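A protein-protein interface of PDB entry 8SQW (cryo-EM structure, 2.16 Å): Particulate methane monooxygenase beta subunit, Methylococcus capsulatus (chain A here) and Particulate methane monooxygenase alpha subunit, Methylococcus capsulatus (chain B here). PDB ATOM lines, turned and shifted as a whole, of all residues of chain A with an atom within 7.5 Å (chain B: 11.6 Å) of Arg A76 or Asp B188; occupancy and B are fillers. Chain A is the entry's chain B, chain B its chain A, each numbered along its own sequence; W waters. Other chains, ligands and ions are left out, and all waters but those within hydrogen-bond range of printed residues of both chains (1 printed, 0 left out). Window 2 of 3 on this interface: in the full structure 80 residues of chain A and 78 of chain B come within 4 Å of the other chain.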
ATOM      1  N   GLN A  70      -4.614  40.631   8.912  1.00  0.00           N
ATOM      2  CA  GLN A  70      -4.228  39.866  10.092  1.00  0.00           C
ATOM      3  C   GLN A  70      -5.276  38.813  10.420  1.00  0.00           C
ATOM      4  O   GLN A  70      -4.950  37.635  10.606  1.00  0.00           O
ATOM      5  CB  GLN A  70      -4.028  40.809  11.274  1.00  0.00           C
ATOM      6  CG  GLN A  70      -2.587  41.147  11.573  1.00  0.00           C
ATOM      7  CD  GLN A  70      -2.447  41.968  12.835  1.00  0.00           C
ATOM      8  OE1 GLN A  70      -3.438  42.431  13.399  1.00  0.00           O
ATOM      9  NE2 GLN A  70      -1.216  42.146  13.289  1.00  0.00           N
ATOM     10  N   SER A  71      -6.551  39.221  10.456  1.00  0.00           N
ATOM     11  CA  SER A  71      -7.630  38.298  10.784  1.00  0.00           C
ATOM     12  C   SER A  71      -7.681  37.126   9.816  1.00  0.00           C
ATOM     13  O   SER A  71      -8.189  36.057  10.162  1.00  0.00           O
ATOM     14  CB  SER A  71      -8.968  39.034  10.784  1.00  0.00           C
ATOM     15  OG  SER A  71      -9.565  39.003   9.497  1.00  0.00           O
ATOM     16  N   TYR A  72      -7.178  37.316   8.600  1.00  0.00           N
ATOM     17  CA  TYR A  72      -7.123  36.194   7.665  1.00  0.00           C
ATOM     18  C   TYR A  72      -5.838  35.386   7.826  1.00  0.00           C
ATOM     19  O   TYR A  72      -5.881  34.168   8.034  1.00  0.00           O
ATOM     20  CB  TYR A  72      -7.259  36.702   6.233  1.00  0.00           C
ATOM     21  CG  TYR A  72      -6.931  35.674   5.176  1.00  0.00           C
ATOM     22  CD1 TYR A  72      -7.785  34.610   4.926  1.00  0.00           C
ATOM     23  CD2 TYR A  72      -5.769  35.775   4.420  1.00  0.00           C
ATOM     24  CE1 TYR A  72      -7.489  33.674   3.955  1.00  0.00           C
ATOM     25  CE2 TYR A  72      -5.469  34.844   3.448  1.00  0.00           C
ATOM     26  CZ  TYR A  72      -6.333  33.794   3.220  1.00  0.00           C
ATOM     27  OH  TYR A  72      -6.035  32.863   2.255  1.00  0.00           O
ATOM     28  N   LEU A  73      -4.686  36.053   7.716  1.00  0.00           N
ATOM     29  CA  LEU A  73      -3.411  35.347   7.666  1.00  0.00           C
ATOM     30  C   LEU A  73      -3.128  34.614   8.969  1.00  0.00           C
ATOM     31  O   LEU A  73      -2.784  33.429   8.957  1.00  0.00           O
ATOM     32  CB  LEU A  73      -2.281  36.327   7.348  1.00  0.00           C
ATOM     33  CG  LEU A  73      -2.159  36.776   5.892  1.00  0.00           C
ATOM     34  CD1 LEU A  73      -0.920  37.632   5.704  1.00  0.00           C
ATOM     35  CD2 LEU A  73      -2.129  35.576   4.957  1.00  0.00           C
ATOM     36  N   TRP A  74      -3.262  35.297  10.108  1.00  0.00           N
ATOM     37  CA  TRP A  74      -2.996  34.634  11.379  1.00  0.00           C
ATOM     38  C   TRP A  74      -3.953  33.469  11.592  1.00  0.00           C
ATOM     39  O   TRP A  74      -3.526  32.353  11.906  1.00  0.00           O
ATOM     40  CB  TRP A  74      -3.094  35.635  12.527  1.00  0.00           C
ATOM     41  CG  TRP A  74      -2.873  35.010  13.866  1.00  0.00           C
ATOM     42  CD1 TRP A  74      -3.804  34.814  14.842  1.00  0.00           C
ATOM     43  CD2 TRP A  74      -1.645  34.470  14.366  1.00  0.00           C
ATOM     44  NE1 TRP A  74      -3.231  34.201  15.928  1.00  0.00           N
ATOM     45  CE2 TRP A  74      -1.905  33.978  15.660  1.00  0.00           C
ATOM     46  CE3 TRP A  74      -0.353  34.363  13.850  1.00  0.00           C
ATOM     47  CZ2 TRP A  74      -0.918  33.387  16.444  1.00  0.00           C
ATOM     48  CZ3 TRP A  74       0.626  33.776  14.629  1.00  0.00           C
ATOM     49  CH2 TRP A  74       0.336  33.295  15.912  1.00  0.00           C
ATOM     50  N   GLU A  75      -5.247  33.697  11.359  1.00  0.00           N
ATOM     51  CA  GLU A  75      -6.242  32.661  11.615  1.00  0.00           C
ATOM     52  C   GLU A  75      -6.031  31.434  10.734  1.00  0.00           C
ATOM     53  O   GLU A  75      -6.213  30.304  11.201  1.00  0.00           O
ATOM     54  CB  GLU A  75      -7.647  33.221  11.410  1.00  0.00           C
ATOM     55  CG  GLU A  75      -8.774  32.308  11.881  1.00  0.00           C
ATOM     56  CD  GLU A  75      -8.774  32.071  13.383  1.00  0.00           C
ATOM     57  OE1 GLU A  75      -8.076  32.805  14.116  1.00  0.00           O
ATOM     58  OE2 GLU A  75      -9.481  31.145  13.833  1.00  0.00           O
ATOM     59  N   ARG A  76      -5.653  31.621   9.469  1.00  0.00           N
ATOM     60  CA  ARG A  76      -5.613  30.501   8.542  1.00  0.00           C
ATOM     61  C   ARG A  76      -4.232  29.881   8.368  1.00  0.00           C
ATOM     62  O   ARG A  76      -4.149  28.718   7.957  1.00  0.00           O
ATOM     63  CB  ARG A  76      -6.145  30.930   7.170  1.00  0.00           C
ATOM     64  CG  ARG A  76      -7.618  31.311   7.168  1.00  0.00           C
ATOM     65  CD  ARG A  76      -8.463  30.307   7.936  1.00  0.00           C
ATOM     66  NE  ARG A  76      -8.394  28.968   7.361  1.00  0.00           N
ATOM     67  CZ  ARG A  76      -9.180  28.531   6.388  1.00  0.00           C
ATOM     68  NH1 ARG A  76     -10.117  29.299   5.859  1.00  0.00           N
ATOM     69  NH2 ARG A  76      -9.026  27.290   5.936  1.00  0.00           N
ATOM     70  N   TYR A  77      -3.149  30.604   8.663  1.00  0.00           N
ATOM     71  CA  TYR A  77      -1.813  30.077   8.438  1.00  0.00           C
ATOM     72  C   TYR A  77      -0.865  30.294   9.609  1.00  0.00           C
ATOM     73  O   TYR A  77       0.274  29.818   9.542  1.00  0.00           O
ATOM     74  CB  TYR A  77      -1.187  30.713   7.182  1.00  0.00           C
ATOM     75  CG  TYR A  77      -2.091  30.795   5.974  1.00  0.00           C
ATOM     76  CD1 TYR A  77      -2.993  31.838   5.823  1.00  0.00           C
ATOM     77  CD2 TYR A  77      -2.029  29.838   4.971  1.00  0.00           C
ATOM     78  CE1 TYR A  77      -3.816  31.919   4.717  1.00  0.00           C
ATOM     79  CE2 TYR A  77      -2.844  29.910   3.864  1.00  0.00           C
ATOM     80  CZ  TYR A  77      -3.737  30.951   3.742  1.00  0.00           C
ATOM     81  OH  TYR A  77      -4.552  31.025   2.638  1.00  0.00           O
ATOM     82  N   ARG A  78      -1.283  30.988  10.669  1.00  0.00           N
ATOM     83  CA  ARG A  78      -0.387  31.408  11.746  1.00  0.00           C
ATOM     84  C   ARG A  78       0.799  32.194  11.196  1.00  0.00           C
ATOM     85  O   ARG A  78       1.941  32.021  11.623  1.00  0.00           O
ATOM     86  CB  ARG A  78       0.077  30.215  12.581  1.00  0.00           C
ATOM     87  CG  ARG A  78      -1.034  29.563  13.376  1.00  0.00           C
ATOM     88  CD  ARG A  78      -1.404  30.407  14.584  1.00  0.00           C
ATOM     89  NE  ARG A  78      -2.554  29.879  15.306  1.00  0.00           N
ATOM     90  CZ  ARG A  78      -3.801  29.892  14.854  1.00  0.00           C
ATOM     91  NH1 ARG A  78      -4.110  30.429  13.685  1.00  0.00           N
ATOM     92  NH2 ARG A  78      -4.765  29.362  15.600  1.00  0.00           N
ATOM     93  N   LEU A  79       0.520  33.070  10.230  1.00  0.00           N
ATOM     94  CA  LEU A  79       1.529  33.967   9.673  1.00  0.00           C
ATOM     95  C   LEU A  79       1.345  35.344  10.290  1.00  0.00           C
ATOM     96  O   LEU A  79       0.389  36.056   9.946  1.00  0.00           O
ATOM     97  CB  LEU A  79       1.408  34.041   8.149  1.00  0.00           C
ATOM     98  CG  LEU A  79       1.913  32.830   7.368  1.00  0.00           C
ATOM     99  CD1 LEU A  79       1.478  32.918   5.919  1.00  0.00           C
ATOM    100  CD2 LEU A  79       3.420  32.722   7.471  1.00  0.00           C
ATOM    101  N   TYR A 135      -7.358  38.135  19.424  1.00  0.00           N
ATOM    102  CA  TYR A 135      -7.680  39.256  18.548  1.00  0.00           C
ATOM    103  C   TYR A 135      -8.228  40.442  19.328  1.00  0.00           C
ATOM    104  O   TYR A 135      -7.974  41.591  18.957  1.00  0.00           O
ATOM    105  CB  TYR A 135      -8.677  38.823  17.473  1.00  0.00           C
ATOM    106  CG  TYR A 135      -8.064  38.007  16.361  1.00  0.00           C
ATOM    107  CD1 TYR A 135      -7.230  38.597  15.423  1.00  0.00           C
ATOM    108  CD2 TYR A 135      -8.317  36.647  16.249  1.00  0.00           C
ATOM    109  CE1 TYR A 135      -6.667  37.859  14.402  1.00  0.00           C
ATOM    110  CE2 TYR A 135      -7.760  35.900  15.237  1.00  0.00           C
ATOM    111  CZ  TYR A 135      -6.936  36.510  14.315  1.00  0.00           C
ATOM    112  OH  TYR A 135      -6.382  35.764  13.306  1.00  0.00           O
ATOM    113  N   ARG A 230     -12.845  38.992   8.159  1.00  0.00           N
ATOM    114  CA  ARG A 230     -13.464  37.685   8.347  1.00  0.00           C
ATOM    115  C   ARG A 230     -14.478  37.404   7.250  1.00  0.00           C
ATOM    116  O   ARG A 230     -14.502  36.311   6.672  1.00  0.00           O
ATOM    117  CB  ARG A 230     -14.130  37.614   9.723  1.00  0.00           C
ATOM    118  CG  ARG A 230     -13.211  37.153  10.831  1.00  0.00           C
ATOM    119  CD  ARG A 230     -12.432  35.920  10.416  1.00  0.00           C
ATOM    120  NE  ARG A 230     -11.101  35.897  11.008  1.00  0.00           N
ATOM    121  CZ  ARG A 230     -10.840  35.521  12.253  1.00  0.00           C
ATOM    122  NH1 ARG A 230     -11.800  35.114  13.065  1.00  0.00           N
ATOM    123  NH2 ARG A 230      -9.587  35.556  12.688  1.00  0.00           N
ATOM    124  N   SER A 233     -12.945  36.768   3.736  1.00  0.00           N
ATOM    125  CA  SER A 233     -12.262  35.456   3.606  1.00  0.00           C
ATOM    126  C   SER A 233     -13.256  34.367   3.185  1.00  0.00           C
ATOM    127  O   SER A 233     -12.789  33.314   2.748  1.00  0.00           O
ATOM    128  CB  SER A 233     -11.564  35.097   4.889  1.00  0.00           C
ATOM    129  OG  SER A 233     -10.540  36.029   5.181  1.00  0.00           O
ATOM    130  N   ASN A 234     -14.566  34.624   3.272  1.00  0.00           N
ATOM    131  CA  ASN A 234     -15.614  33.606   2.957  1.00  0.00           C
ATOM    132  C   ASN A 234     -15.238  32.762   1.730  1.00  0.00           C
ATOM    133  O   ASN A 234     -14.811  33.340   0.714  1.00  0.00           O
ATOM    134  CB  ASN A 234     -17.006  34.245   2.833  1.00  0.00           C
ATOM    135  CG  ASN A 234     -17.358  34.721   1.439  1.00  0.00           C
ATOM    136  OD1 ASN A 234     -17.965  33.988   0.665  1.00  0.00           O
ATOM    137  ND2 ASN A 234     -16.982  35.947   1.111  1.00  0.00           N
ATOM    138  N   GLU A 235     -15.384  31.438   1.829  1.00  0.00           N
ATOM    139  CA  GLU A 235     -15.128  30.551   0.699  1.00  0.00           C
ATOM    140  C   GLU A 235     -16.431  30.020   0.120  1.00  0.00           C
ATOM    141  O   GLU A 235     -16.496  28.896  -0.387  1.00  0.00           O
ATOM    142  CB  GLU A 235     -14.222  29.394   1.111  1.00  0.00           C
ATOM    143  CG  GLU A 235     -12.905  29.820   1.727  1.00  0.00           C
ATOM    144  CD  GLU A 235     -12.508  28.952   2.904  1.00  0.00           C
ATOM    145  OE1 GLU A 235     -12.694  27.720   2.828  1.00  0.00           O
ATOM    146  OE2 GLU A 235     -12.015  29.503   3.910  1.00  0.00           O
ATOM    147  N   PRO B 178       8.245  27.152   4.728  1.00  0.00           N
ATOM    148  CA  PRO B 178       7.110  27.156   3.797  1.00  0.00           C
ATOM    149  C   PRO B 178       5.971  28.024   4.313  1.00  0.00           C
ATOM    150  O   PRO B 178       5.722  28.109   5.517  1.00  0.00           O
ATOM    151  CB  PRO B 178       6.712  25.677   3.716  1.00  0.00           C
ATOM    152  CG  PRO B 178       7.444  24.996   4.839  1.00  0.00           C
ATOM    153  CD  PRO B 178       8.693  25.782   5.023  1.00  0.00           C
ATOM    154  N   ILE B 179       5.271  28.676   3.382  1.00  0.00           N
ATOM    155  CA  ILE B 179       4.419  29.807   3.737  1.00  0.00           C
ATOM    156  C   ILE B 179       2.935  29.465   3.751  1.00  0.00           C
ATOM    157  O   ILE B 179       2.280  29.566   4.792  1.00  0.00           O
ATOM    158  CB  ILE B 179       4.680  30.991   2.789  1.00  0.00           C
ATOM    159  CG1 ILE B 179       6.161  31.370   2.802  1.00  0.00           C
ATOM    160  CG2 ILE B 179       3.819  32.184   3.174  1.00  0.00           C
ATOM    161  CD1 ILE B 179       6.569  32.250   1.646  1.00  0.00           C
ATOM    162  N   PHE B 180       2.369  29.087   2.602  1.00  0.00           N
ATOM    163  CA  PHE B 180       0.916  29.132   2.462  1.00  0.00           C
ATOM    164  C   PHE B 180       0.228  27.778   2.610  1.00  0.00           C
ATOM    165  O   PHE B 180      -0.561  27.587   3.538  1.00  0.00           O
ATOM    166  CB  PHE B 180       0.555  29.755   1.108  1.00  0.00           C
ATOM    167  CG  PHE B 180       0.703  31.246   1.076  1.00  0.00           C
ATOM    168  CD1 PHE B 180      -0.098  32.050   1.870  1.00  0.00           C
ATOM    169  CD2 PHE B 180       1.643  31.844   0.258  1.00  0.00           C
ATOM    170  CE1 PHE B 180       0.038  33.422   1.845  1.00  0.00           C
ATOM    171  CE2 PHE B 180       1.784  33.216   0.231  1.00  0.00           C
ATOM    172  CZ  PHE B 180       0.980  34.007   1.026  1.00  0.00           C
ATOM    173  N   ILE B 181       0.527  26.823   1.739  1.00  0.00           N
ATOM    174  CA  ILE B 181      -0.322  25.635   1.646  1.00  0.00           C
ATOM    175  C   ILE B 181      -0.033  24.658   2.782  1.00  0.00           C
ATOM    176  O   ILE B 181      -0.987  24.174   3.413  1.00  0.00           O
ATOM    177  CB  ILE B 181      -0.189  24.954   0.273  1.00  0.00           C
ATOM    178  CG1 ILE B 181      -0.786  25.848  -0.818  1.00  0.00           C
ATOM    179  CG2 ILE B 181      -0.918  23.628   0.280  1.00  0.00           C
ATOM    180  CD1 ILE B 181      -1.074  25.125  -2.116  1.00  0.00           C
ATOM    181  N   PRO B 182       1.226  24.303   3.075  1.00  0.00           N
ATOM    182  CA  PRO B 182       1.455  23.431   4.241  1.00  0.00           C
ATOM    183  C   PRO B 182       0.983  24.036   5.551  1.00  0.00           C
ATOM    184  O   PRO B 182       0.440  23.315   6.394  1.00  0.00           O
ATOM    185  CB  PRO B 182       2.975  23.213   4.223  1.00  0.00           C
ATOM    186  CG  PRO B 182       3.516  24.313   3.401  1.00  0.00           C
ATOM    187  CD  PRO B 182       2.486  24.587   2.368  1.00  0.00           C
ATOM    188  N   ARG B 183       1.151  25.347   5.740  1.00  0.00           N
ATOM    189  CA  ARG B 183       0.667  25.973   6.970  1.00  0.00           C
ATOM    190  C   ARG B 183      -0.853  25.957   7.030  1.00  0.00           C
ATOM    191  O   ARG B 183      -1.436  25.723   8.096  1.00  0.00           O
ATOM    192  CB  ARG B 183       1.199  27.402   7.088  1.00  0.00           C
ATOM    193  CG  ARG B 183       2.679  27.485   7.416  1.00  0.00           C
ATOM    194  CD  ARG B 183       3.137  28.917   7.621  1.00  0.00           C
ATOM    195  NE  ARG B 183       2.910  29.380   8.984  1.00  0.00           N
ATOM    196  CZ  ARG B 183       3.808  29.309   9.957  1.00  0.00           C
ATOM    197  NH1 ARG B 183       5.004  28.779   9.755  1.00  0.00           N
ATOM    198  NH2 ARG B 183       3.500  29.782  11.160  1.00  0.00           N
ATOM    199  N   LEU B 184      -1.515  26.200   5.895  1.00  0.00           N
ATOM    200  CA  LEU B 184      -2.971  26.120   5.850  1.00  0.00           C
ATOM    201  C   LEU B 184      -3.451  24.717   6.197  1.00  0.00           C
ATOM    202  O   LEU B 184      -4.406  24.551   6.965  1.00  0.00           O
ATOM    203  CB  LEU B 184      -3.464  26.524   4.462  1.00  0.00           C
ATOM    204  CG  LEU B 184      -4.939  26.301   4.130  1.00  0.00           C
ATOM    205  CD1 LEU B 184      -5.811  27.278   4.897  1.00  0.00           C
ATOM    206  CD2 LEU B 184      -5.174  26.425   2.635  1.00  0.00           C
ATOM    207  N   LEU B 185      -2.796  23.697   5.637  1.00  0.00           N
ATOM    208  CA  LEU B 185      -3.178  22.320   5.929  1.00  0.00           C
ATOM    209  C   LEU B 185      -2.938  21.975   7.395  1.00  0.00           C
ATOM    210  O   LEU B 185      -3.747  21.276   8.012  1.00  0.00           O
ATOM    211  CB  LEU B 185      -2.411  21.357   5.022  1.00  0.00           C
ATOM    212  CG  LEU B 185      -2.809  21.363   3.546  1.00  0.00           C
ATOM    213  CD1 LEU B 185      -1.859  20.500   2.734  1.00  0.00           C
ATOM    214  CD2 LEU B 185      -4.240  20.899   3.372  1.00  0.00           C
ATOM    215  N   MET B 186      -1.829  22.448   7.964  1.00  0.00           N
ATOM    216  CA  MET B 186      -1.559  22.195   9.376  1.00  0.00           C
ATOM    217  C   MET B 186      -2.601  22.856  10.268  1.00  0.00           C
ATOM    218  O   MET B 186      -3.050  22.258  11.252  1.00  0.00           O
ATOM    219  CB  MET B 186      -0.157  22.684   9.738  1.00  0.00           C
ATOM    220  CG  MET B 186       0.958  21.787   9.237  1.00  0.00           C
ATOM    221  SD  MET B 186       1.158  20.313  10.251  1.00  0.00           S
ATOM    222  CE  MET B 186       1.722  21.040  11.787  1.00  0.00           C
ATOM    223  N   VAL B 187      -2.991  24.090   9.945  1.00  0.00           N
ATOM    224  CA  VAL B 187      -3.997  24.778  10.752  1.00  0.00           C
ATOM    225  C   VAL B 187      -5.350  24.090  10.628  1.00  0.00           C
ATOM    226  O   VAL B 187      -6.065  23.917  11.623  1.00  0.00           O
ATOM    227  CB  VAL B 187      -4.075  26.264  10.358  1.00  0.00           C
ATOM    228  CG1 VAL B 187      -5.264  26.929  11.028  1.00  0.00           C
ATOM    229  CG2 VAL B 187      -2.788  26.981  10.737  1.00  0.00           C
ATOM    230  N   ASP B 188      -5.726  23.680   9.413  1.00  0.00           N
ATOM    231  CA  ASP B 188      -7.032  23.055   9.203  1.00  0.00           C
ATOM    232  C   ASP B 188      -7.100  21.672   9.846  1.00  0.00           C
ATOM    233  O   ASP B 188      -7.953  21.408  10.698  1.00  0.00           O
ATOM    234  CB  ASP B 188      -7.339  22.971   7.706  1.00  0.00           C
ATOM    235  CG  ASP B 188      -7.659  24.322   7.099  1.00  0.00           C
ATOM    236  OD1 ASP B 188      -8.305  25.145   7.781  1.00  0.00           O
ATOM    237  OD2 ASP B 188      -7.269  24.560   5.938  1.00  0.00           O
ATOM    238  N   ALA B 189      -6.201  20.775   9.443  1.00  0.00           N
ATOM    239  CA  ALA B 189      -6.219  19.404   9.939  1.00  0.00           C
ATOM    240  C   ALA B 189      -5.676  19.340  11.358  1.00  0.00           C
ATOM    241  O   ALA B 189      -4.465  19.221  11.565  1.00  0.00           O
ATOM    242  CB  ALA B 189      -5.416  18.488   9.018  1.00  0.00           C
ATOM    243  N   GLY B 190      -6.569  19.419  12.341  1.00  0.00           N
ATOM    244  CA  GLY B 190      -6.173  19.383  13.731  1.00  0.00           C
ATOM    245  C   GLY B 190      -5.652  20.721  14.216  1.00  0.00           C
ATOM    246  O   GLY B 190      -5.537  21.697  13.474  1.00  0.00           O
ATOM    247  N   ARG B 191      -5.332  20.756  15.506  1.00  0.00           N
ATOM    248  CA  ARG B 191      -4.740  21.947  16.092  1.00  0.00           C
ATOM    249  C   ARG B 191      -3.340  22.154  15.525  1.00  0.00           C
ATOM    250  O   ARG B 191      -2.585  21.203  15.308  1.00  0.00           O
ATOM    251  CB  ARG B 191      -4.677  21.810  17.613  1.00  0.00           C
ATOM    252  CG  ARG B 191      -6.007  22.026  18.311  1.00  0.00           C
ATOM    253  CD  ARG B 191      -5.894  21.713  19.793  1.00  0.00           C
ATOM    254  NE  ARG B 191      -7.143  21.958  20.501  1.00  0.00           N
ATOM    255  CZ  ARG B 191      -7.593  21.212  21.500  1.00  0.00           C
ATOM    256  NH1 ARG B 191      -6.912  20.165  21.939  1.00  0.00           N
ATOM    257  NH2 ARG B 191      -8.755  21.518  22.068  1.00  0.00           N
ATOM    258  N   ALA B 192      -2.992  23.416  15.275  1.00  0.00           N
ATOM    259  CA  ALA B 192      -1.694  23.651  14.657  1.00  0.00           C
ATOM    260  C   ALA B 192      -0.587  23.636  15.697  1.00  0.00           C
ATOM    261  O   ALA B 192       0.187  22.676  15.765  1.00  0.00           O
ATOM    262  CB  ALA B 192      -1.699  24.986  13.911  1.00  0.00           C
ATOM    263  N   ASP B 193      -0.525  24.682  16.524  1.00  0.00           N
ATOM    264  CA  ASP B 193       0.305  24.749  17.732  1.00  0.00           C
ATOM    265  C   ASP B 193       1.715  24.196  17.512  1.00  0.00           C
ATOM    266  O   ASP B 193       2.378  23.723  18.436  1.00  0.00           O
ATOM    267  CB  ASP B 193      -0.380  24.032  18.893  1.00  0.00           C
ATOM    268  CG  ASP B 193      -1.575  24.798  19.424  1.00  0.00           C
ATOM    269  OD1 ASP B 193      -1.587  26.040  19.299  1.00  0.00           O
ATOM    270  OD2 ASP B 193      -2.500  24.157  19.962  1.00  0.00           O
ATOM    271  N   GLU B 194       2.179  24.255  16.263  1.00  0.00           N
ATOM    272  CA  GLU B 194       3.478  23.683  15.933  1.00  0.00           C
ATOM    273  C   GLU B 194       4.277  24.605  15.028  1.00  0.00           C
ATOM    274  O   GLU B 194       5.510  24.531  14.984  1.00  0.00           O
ATOM    275  CB  GLU B 194       3.303  22.313  15.277  1.00  0.00           C
ATOM    276  CG  GLU B 194       3.133  21.174  16.269  1.00  0.00           C
ATOM    277  CD  GLU B 194       2.156  20.119  15.788  1.00  0.00           C
ATOM    278  OE1 GLU B 194       2.386  19.547  14.703  1.00  0.00           O
ATOM    279  OE2 GLU B 194       1.159  19.861  16.496  1.00  0.00           O
ATOM    280  N   LEU B 195       3.584  25.474  14.293  1.00  0.00           N
ATOM    281  CA  LEU B 195       4.250  26.387  13.381  1.00  0.00           C
ATOM    282  C   LEU B 195       4.667  27.689  14.052  1.00  0.00           C
ATOM    283  O   LEU B 195       5.409  28.471  13.447  1.00  0.00           O
ATOM    284  CB  LEU B 195       3.350  26.679  12.179  1.00  0.00           C
ATOM    285  CG  LEU B 195       2.680  25.431  11.600  1.00  0.00           C
ATOM    286  CD1 LEU B 195       1.207  25.405  11.960  1.00  0.00           C
ATOM    287  CD2 LEU B 195       2.875  25.318  10.103  1.00  0.00           C
ATOM    288  N   VAL B 196       4.206  27.935  15.273  1.00  0.00           N
ATOM    289  CA  VAL B 196       4.664  29.073  16.060  1.00  0.00           C
ATOM    290  C   VAL B 196       5.148  28.551  17.405  1.00  0.00           C
ATOM    291  O   VAL B 196       4.357  28.343  18.332  1.00  0.00           O
ATOM    292  CB  VAL B 196       3.555  30.127  16.234  1.00  0.00           C
ATOM    293  CG1 VAL B 196       4.009  31.235  17.173  1.00  0.00           C
ATOM    294  CG2 VAL B 196       3.151  30.699  14.883  1.00  0.00           C
HETATM  295  O   HOH W   1      -6.543  26.972   8.144  1.00  0.00           O
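Water W1 lies within hydrogen-bond range of the side-chain carboxylate (OD1) of Asp B188 (2.6 Å), the guanidinium group (NE) of Arg A76 (2.8 Å) and the backbone carbonyl oxygen (O) of Leu B184 (3.4 Å).
Of the 19 printed residues of chain B, 7 touch a printed residue of chain A. Hydrophobic or aromatic side chains of chain B within 4 Å of the printed part of chain A: Ile B179, Leu B184, Val B187 and Val B196. Printed residues of chain A that touch a printed residue of chain B: Trp A74, Glu A75, Arg A76, Tyr A77, Arg A78 and Leu A79. Hydrophobic or aromatic side chains of chain A within 4 Å of the printed part of chain B: Trp A74, Tyr A77 and Leu A79. Among the printed residues, Asp or Glu carboxylates within 4 Å of a Lys or Arg side-chain nitrogen of the other chain: Arg A76 with Asp B188 (2.9 Å).
The backbone carbonyl oxygen of Glu A75 sits at hydrogen-bond distance from the guanidinium group of Arg A78, at 3.3 Å. The side-chain carboxylate (OE1) of Glu A75 lies within salt-bridge range of the guanidinium group (NH2) of Arg A230 (3.4 Å). N of Glu A75 sits at hydrogen-bond distance from OH of Tyr A135, at 3.1 Å. N of Arg A78 lies within hydrogen-bond range of O of Leu A73 (3.3 Å). NH1 of Arg A76 is in salt-bridge range of OE2 of Glu A235 (2.7 Å). The backbone carbonyl oxygen (O) of Trp A74 lies within hydrogen-bond range of the guanidinium group (NH1) of Arg A78 (2.7 Å).
Of chain B, only Leu B184, Val B187 and Asp B188 come within 4 Å of Arg A76. Asp B188 touches just one residue of chain A: Arg A76. No residue of chain B comes within 4 Å of Tyr A72. Arg A78 touches just these residues of chain B: Arg B183 and Val B196. Printed residues of chain A within 4 Å of Leu B184: Arg A76 and Tyr A77. Of the printed residues of chain A, Ile B179 touches Leu A79 (3.6 Å). Of the printed residues of chain A, Val B187 touches Glu A75, Arg A76 and Tyr A77. Printed residues of chain A within 4 Å of Arg B183: Tyr A77, Arg A78 and Leu A79. Pro B178 touches none of the printed residues of chain A. The nearest residue of chain B that does not touch Arg A76 is Arg B183 (4.04 Å). The nearest residue of chain A that does not touch Asp B188 is Glu A75 (6.5 Å). The nearest printed residue of chain A that does not touch Arg B183 is Arg A76 (4.04 Å).
Val B196 touches Trp A74 (CG2 to CH2, 3.97 Å). CG1 of Val B187 touches O of Glu A75 (3.5 Å). CD1 of Leu B184 touches NH2 of Arg A76, at 3.4 Å. O of Arg A76 touches CB of Val B187 (3.4 Å). CD2 of Tyr A77 touches O of Phe B180, at 3.0 Å. Leu B184 touches Tyr A77. Tyr A77 touches Val B187. O of Arg A78 touches CG2 of Val B196, 3.7 Å away. Ile B179 touches Leu A79. Arg B183 touches Leu A79 (NE to CD2, 3.7 Å).
The guanidinium group of Arg B183 is in hydrogen-bond range of the backbone carbonyl oxygen of Arg A78 (2.8 Å). OD1 of Asp B188 lies within salt-bridge range of NH2 of Arg A76, 2.9 Å away. NE of Arg B183 lies within hydrogen-bond range of O of Tyr A77 (2.7 Å).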
